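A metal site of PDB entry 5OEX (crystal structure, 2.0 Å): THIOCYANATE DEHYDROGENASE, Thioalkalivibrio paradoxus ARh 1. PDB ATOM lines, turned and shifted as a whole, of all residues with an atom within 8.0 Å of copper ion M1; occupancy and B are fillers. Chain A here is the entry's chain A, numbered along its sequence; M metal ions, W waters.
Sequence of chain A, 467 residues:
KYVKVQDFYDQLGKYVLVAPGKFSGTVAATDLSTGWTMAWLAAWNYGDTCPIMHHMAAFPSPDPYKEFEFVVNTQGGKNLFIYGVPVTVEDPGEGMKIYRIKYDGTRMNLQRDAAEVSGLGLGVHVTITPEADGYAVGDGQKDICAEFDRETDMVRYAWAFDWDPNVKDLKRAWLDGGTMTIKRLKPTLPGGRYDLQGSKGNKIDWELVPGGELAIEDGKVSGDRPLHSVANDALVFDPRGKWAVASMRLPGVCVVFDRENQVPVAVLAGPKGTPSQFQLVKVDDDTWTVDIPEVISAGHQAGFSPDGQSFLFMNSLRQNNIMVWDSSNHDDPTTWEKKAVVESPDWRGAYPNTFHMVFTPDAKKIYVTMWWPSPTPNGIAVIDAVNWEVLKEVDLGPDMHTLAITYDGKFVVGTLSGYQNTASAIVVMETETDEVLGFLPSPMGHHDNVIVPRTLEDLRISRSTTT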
ATOM      1  N   HIS A  54      34.768   8.982 -21.688  1.00  0.00           N
ATOM      2  CA  HIS A  54      33.964   7.923 -22.331  1.00  0.00           C
ATOM      3  C   HIS A  54      33.869   7.987 -23.879  1.00  0.00           C
ATOM      4  O   HIS A  54      34.709   7.419 -24.580  1.00  0.00           O
ATOM      5  CB  HIS A  54      32.593   7.703 -21.667  1.00  0.00           C
ATOM      6  CG  HIS A  54      31.988   6.397 -22.065  1.00  0.00           C
ATOM      7  ND1 HIS A  54      30.636   6.150 -22.043  1.00  0.00           N
ATOM      8  CD2 HIS A  54      32.585   5.262 -22.512  1.00  0.00           C
ATOM      9  CE1 HIS A  54      30.408   4.906 -22.439  1.00  0.00           C
ATOM     10  NE2 HIS A  54      31.582   4.372 -22.786  1.00  0.00           N
ATOM     11  N   HIS A  55      32.915   8.729 -24.438  1.00  0.00           N
ATOM     12  CA  HIS A  55      32.867   8.777 -25.852  1.00  0.00           C
ATOM     13  C   HIS A  55      33.279  10.141 -26.294  1.00  0.00           C
ATOM     14  O   HIS A  55      33.340  11.022 -25.441  1.00  0.00           O
ATOM     15  CB  HIS A  55      31.483   8.466 -26.328  1.00  0.00           C
ATOM     16  CG  HIS A  55      31.194   7.012 -26.215  1.00  0.00           C
ATOM     17  ND1 HIS A  55      31.847   6.092 -26.993  1.00  0.00           N
ATOM     18  CD2 HIS A  55      30.385   6.317 -25.370  1.00  0.00           C
ATOM     19  CE1 HIS A  55      31.431   4.877 -26.681  1.00  0.00           C
ATOM     20  NE2 HIS A  55      30.552   4.987 -25.709  1.00  0.00           N
ATOM     21  N   VAL A 124      26.830   8.420 -22.630  1.00  0.00           N
ATOM     22  CA  VAL A 124      27.105   7.385 -23.651  1.00  0.00           C
ATOM     23  C   VAL A 124      27.564   8.085 -24.931  1.00  0.00           C
ATOM     24  O   VAL A 124      28.464   8.948 -24.826  1.00  0.00           O
ATOM     25  CB  VAL A 124      26.015   6.275 -23.715  1.00  0.00           C
ATOM     26  CG1 VAL A 124      26.556   5.007 -24.414  1.00  0.00           C
ATOM     27  CG2 VAL A 124      25.628   5.889 -22.256  1.00  0.00           C
ATOM     28  N   HIS A 125      27.049   7.737 -26.101  1.00  0.00           N
ATOM     29  CA  HIS A 125      27.745   8.154 -27.369  1.00  0.00           C
ATOM     30  C   HIS A 125      27.595   9.613 -27.666  1.00  0.00           C
ATOM     31  O   HIS A 125      26.518  10.181 -27.419  1.00  0.00           O
ATOM     32  CB  HIS A 125      27.199   7.360 -28.588  1.00  0.00           C
ATOM     33  CG  HIS A 125      27.662   5.932 -28.618  1.00  0.00           C
ATOM     34  ND1 HIS A 125      28.917   5.573 -29.008  1.00  0.00           N
ATOM     35  CD2 HIS A 125      27.044   4.777 -28.242  1.00  0.00           C
ATOM     36  CE1 HIS A 125      29.067   4.269 -28.902  1.00  0.00           C
ATOM     37  NE2 HIS A 125      27.957   3.763 -28.436  1.00  0.00           N
ATOM     38  N   GLU A 207      25.728   1.852 -16.895  1.00  0.00           N
ATOM     39  CA  GLU A 207      25.378   1.551 -18.286  1.00  0.00           C
ATOM     40  C   GLU A 207      25.391   0.014 -18.433  1.00  0.00           C
ATOM     41  O   GLU A 207      26.308  -0.616 -17.883  1.00  0.00           O
ATOM     42  CB  GLU A 207      26.465   2.104 -19.224  1.00  0.00           C
ATOM     43  CG  GLU A 207      26.126   1.941 -20.729  1.00  0.00           C
ATOM     44  CD  GLU A 207      27.328   2.246 -21.680  1.00  0.00           C
ATOM     45  OE1 GLU A 207      28.429   2.578 -21.210  1.00  0.00           O
ATOM     46  OE2 GLU A 207      27.190   2.072 -22.915  1.00  0.00           O
ATOM     47  N   ASN A 232      18.789   3.639 -24.170  1.00  0.00           N
ATOM     48  CA  ASN A 232      19.248   4.455 -25.289  1.00  0.00           C
ATOM     49  C   ASN A 232      20.795   4.409 -25.335  1.00  0.00           C
ATOM     50  O   ASN A 232      21.467   4.316 -24.292  1.00  0.00           O
ATOM     51  CB  ASN A 232      18.746   5.890 -25.116  1.00  0.00           C
ATOM     52  CG  ASN A 232      19.283   6.836 -26.194  1.00  0.00           C
ATOM     53  OD1 ASN A 232      20.004   7.802 -25.893  1.00  0.00           O
ATOM     54  ND2 ASN A 232      18.993   6.545 -27.456  1.00  0.00           N
ATOM     55  N   ASP A 233      21.358   4.433 -26.531  1.00  0.00           N
ATOM     56  CA  ASP A 233      22.841   4.263 -26.670  1.00  0.00           C
ATOM     57  C   ASP A 233      23.392   5.487 -27.394  1.00  0.00           C
ATOM     58  O   ASP A 233      24.300   6.151 -26.890  1.00  0.00           O
ATOM     59  CB  ASP A 233      23.101   2.882 -27.345  1.00  0.00           C
ATOM     60  CG  ASP A 233      24.577   2.658 -27.807  1.00  0.00           C
ATOM     61  OD1 ASP A 233      24.759   2.700 -29.068  1.00  0.00           O
ATOM     62  OD2 ASP A 233      25.513   2.332 -27.002  1.00  0.00           O
ATOM     63  N   ALA A 234      22.723   5.876 -28.482  1.00  0.00           N
ATOM     64  CA  ALA A 234      23.213   6.925 -29.384  1.00  0.00           C
ATOM     65  C   ALA A 234      22.128   7.721 -30.129  1.00  0.00           C
ATOM     66  O   ALA A 234      20.990   7.255 -30.314  1.00  0.00           O
ATOM     67  CB  ALA A 234      24.204   6.333 -30.403  1.00  0.00           C
ATOM     68  N   SER A 247      18.996   5.000 -30.965  1.00  0.00           N
ATOM     69  CA  SER A 247      18.940   3.536 -30.805  1.00  0.00           C
ATOM     70  C   SER A 247      18.572   3.140 -29.372  1.00  0.00           C
ATOM     71  O   SER A 247      19.039   3.765 -28.410  1.00  0.00           O
ATOM     72  CB  SER A 247      20.275   2.907 -31.187  1.00  0.00           C
ATOM     73  OG  SER A 247      21.309   3.596 -30.488  1.00  0.00           O
ATOM     74  N   ARG A 249      18.652  -0.064 -26.945  1.00  0.00           N
ATOM     75  CA  ARG A 249      19.193  -1.405 -26.810  1.00  0.00           C
ATOM     76  C   ARG A 249      18.144  -2.434 -26.353  1.00  0.00           C
ATOM     77  O   ARG A 249      17.939  -3.392 -27.058  1.00  0.00           O
ATOM     78  CB  ARG A 249      20.432  -1.407 -25.972  1.00  0.00           C
ATOM     79  CG  ARG A 249      21.607  -0.597 -26.583  1.00  0.00           C
ATOM     80  CD  ARG A 249      22.747  -0.496 -25.571  1.00  0.00           C
ATOM     81  NE  ARG A 249      23.143  -1.835 -25.114  1.00  0.00           N
ATOM     82  CZ  ARG A 249      23.970  -2.090 -24.100  1.00  0.00           C
ATOM     83  NH1 ARG A 249      24.515  -1.092 -23.413  1.00  0.00           N
ATOM     84  NH2 ARG A 249      24.255  -3.339 -23.741  1.00  0.00           N
ATOM     85  N   GLY A 299      19.425  -4.915 -29.364  1.00  0.00           N
ATOM     86  CA  GLY A 299      20.300  -4.439 -30.446  1.00  0.00           C
ATOM     87  C   GLY A 299      21.337  -3.415 -29.938  1.00  0.00           C
ATOM     88  O   GLY A 299      21.278  -2.955 -28.814  1.00  0.00           O
ATOM     89  N   HIS A 300      22.298  -3.027 -30.742  1.00  0.00           N
ATOM     90  CA  HIS A 300      23.240  -2.011 -30.274  1.00  0.00           C
ATOM     91  C   HIS A 300      23.646  -1.028 -31.345  1.00  0.00           C
ATOM     92  O   HIS A 300      23.019   0.001 -31.479  1.00  0.00           O
ATOM     93  CB  HIS A 300      24.501  -2.627 -29.646  1.00  0.00           C
ATOM     94  CG  HIS A 300      25.303  -1.669 -28.819  1.00  0.00           C
ATOM     95  ND1 HIS A 300      25.801  -2.008 -27.570  1.00  0.00           N
ATOM     96  CD2 HIS A 300      25.712  -0.392 -29.054  1.00  0.00           C
ATOM     97  CE1 HIS A 300      26.475  -0.978 -27.071  1.00  0.00           C
ATOM     98  NE2 HIS A 300      26.416   0.016 -27.928  1.00  0.00           N
ATOM     99  N   GLN A 301      24.704  -1.342 -32.090  1.00  0.00           N
ATOM    100  CA  GLN A 301      25.244  -0.419 -33.081  1.00  0.00           C
ATOM    101  C   GLN A 301      24.229   0.027 -34.116  1.00  0.00           C
ATOM    102  O   GLN A 301      23.429  -0.800 -34.601  1.00  0.00           O
ATOM    103  CB  GLN A 301      26.452  -1.103 -33.748  1.00  0.00           C
ATOM    104  CG  GLN A 301      27.015  -0.464 -35.037  1.00  0.00           C
ATOM    105  CD  GLN A 301      27.389   1.013 -34.856  1.00  0.00           C
ATOM    106  OE1 GLN A 301      27.865   1.401 -33.785  1.00  0.00           O
ATOM    107  NE2 GLN A 301      27.145   1.836 -35.882  1.00  0.00           N
ATOM    108  N   ALA A 302      24.244   1.307 -34.490  1.00  0.00           N
ATOM    109  CA  ALA A 302      23.275   1.851 -35.468  1.00  0.00           C
ATOM    110  C   ALA A 302      23.932   2.896 -36.353  1.00  0.00           C
ATOM    111  O   ALA A 302      24.657   3.731 -35.876  1.00  0.00           O
ATOM    112  CB  ALA A 302      22.137   2.485 -34.718  1.00  0.00           C
ATOM    113  N   PHE A 355      29.779  -4.001 -32.047  1.00  0.00           N
ATOM    114  CA  PHE A 355      29.169  -2.724 -31.513  1.00  0.00           C
ATOM    115  C   PHE A 355      29.631  -1.468 -32.226  1.00  0.00           C
ATOM    116  O   PHE A 355      29.198  -0.319 -31.872  1.00  0.00           O
ATOM    117  CB  PHE A 355      29.451  -2.487 -30.013  1.00  0.00           C
ATOM    118  CG  PHE A 355      29.026  -3.596 -29.114  1.00  0.00           C
ATOM    119  CD1 PHE A 355      27.717  -4.120 -29.164  1.00  0.00           C
ATOM    120  CD2 PHE A 355      29.912  -4.098 -28.157  1.00  0.00           C
ATOM    121  CE1 PHE A 355      27.313  -5.159 -28.314  1.00  0.00           C
ATOM    122  CE2 PHE A 355      29.504  -5.125 -27.314  1.00  0.00           C
ATOM    123  CZ  PHE A 355      28.193  -5.645 -27.383  1.00  0.00           C
ATOM    124  N   HIS A 356      30.562  -1.653 -33.151  1.00  0.00           N
ATOM    125  CA  HIS A 356      31.195  -0.495 -33.809  1.00  0.00           C
ATOM    126  C   HIS A 356      31.428  -0.782 -35.300  1.00  0.00           C
ATOM    127  O   HIS A 356      31.723  -1.932 -35.708  1.00  0.00           O
ATOM    128  CB  HIS A 356      32.485  -0.070 -33.074  1.00  0.00           C
ATOM    129  CG  HIS A 356      32.326   0.158 -31.586  1.00  0.00           C
ATOM    130  ND1 HIS A 356      31.709   1.273 -31.079  1.00  0.00           N
ATOM    131  CD2 HIS A 356      32.717  -0.559 -30.494  1.00  0.00           C
ATOM    132  CE1 HIS A 356      31.723   1.250 -29.748  1.00  0.00           C
ATOM    133  NE2 HIS A 356      32.365   0.167 -29.359  1.00  0.00           N
ATOM    134  N   THR A 402      36.392   0.828 -30.820  1.00  0.00           N
ATOM    135  CA  THR A 402      35.988   1.568 -32.008  1.00  0.00           C
ATOM    136  C   THR A 402      36.946   1.478 -33.194  1.00  0.00           C
ATOM    137  O   THR A 402      38.084   1.031 -33.059  1.00  0.00           O
ATOM    138  CB  THR A 402      35.699   3.033 -31.672  1.00  0.00           C
ATOM    139  OG1 THR A 402      36.787   3.487 -30.839  1.00  0.00           O
ATOM    140  CG2 THR A 402      34.327   3.118 -30.967  1.00  0.00           C
ATOM    141  N   HIS A 447      37.115   3.624 -25.179  1.00  0.00           N
ATOM    142  CA  HIS A 447      35.924   3.161 -25.812  1.00  0.00           C
ATOM    143  C   HIS A 447      35.511   4.029 -27.011  1.00  0.00           C
ATOM    144  O   HIS A 447      34.348   3.974 -27.500  1.00  0.00           O
ATOM    145  CB  HIS A 447      34.779   3.098 -24.781  1.00  0.00           C
ATOM    146  CG  HIS A 447      34.883   1.928 -23.858  1.00  0.00           C
ATOM    147  ND1 HIS A 447      33.798   1.442 -23.174  1.00  0.00           N
ATOM    148  CD2 HIS A 447      35.933   1.124 -23.514  1.00  0.00           C
ATOM    149  CE1 HIS A 447      34.183   0.436 -22.388  1.00  0.00           C
ATOM    150  NE2 HIS A 447      35.459   0.186 -22.620  1.00  0.00           N
ATOM    151  N   THR A 467      28.502   4.835 -34.808  1.00  0.00           N
ATOM    152  CA  THR A 467      29.334   4.738 -33.592  1.00  0.00           C
ATOM    153  C   THR A 467      30.354   3.548 -33.594  1.00  0.00           C
ATOM    154  O   THR A 467      31.090   3.387 -32.565  1.00  0.00           O
ATOM    155  CB  THR A 467      28.474   4.755 -32.292  1.00  0.00           C
ATOM    156  OG1 THR A 467      27.659   3.596 -32.168  1.00  0.00           O
ATOM    157  CG2 THR A 467      27.596   6.023 -32.240  1.00  0.00           C
ATOM    158  OXT THR A 467      30.503   2.768 -34.599  1.00  0.00           O
HETATM  159 CU    CU M   1      27.190   1.893 -28.135  1.00  0.00          CU
HETATM  160 CU    CU M   2      33.392   0.674 -27.499  1.00  0.00          CU
HETATM  161 CU    CU M   3      31.912   2.389 -23.561  1.00  0.00          CU
HETATM  162 CU    CU M   4      32.305   2.536 -22.514  1.00  0.00          CU
HETATM  163  O   HOH W   1      28.095   1.609 -30.023  1.00  0.00           O
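Copper ion M1 is bound by NE2 of His 300 (2.0 Å), NE2 of His 125 (2.0 Å), OD2 of Asp 233 (2.1 Å) and water W1 (2.1 Å). Slightly farther from copper ion M1 lies OD1 of Asp 233 (2.7 Å).
Water W1 bridges O of Phe 355 and OG1 of Thr 467.
The backbone NH (N) of Asp 233 is in hydrogen-bond range of the backbone carbonyl oxygen (O) of Ser 247, at 3.1 Å.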
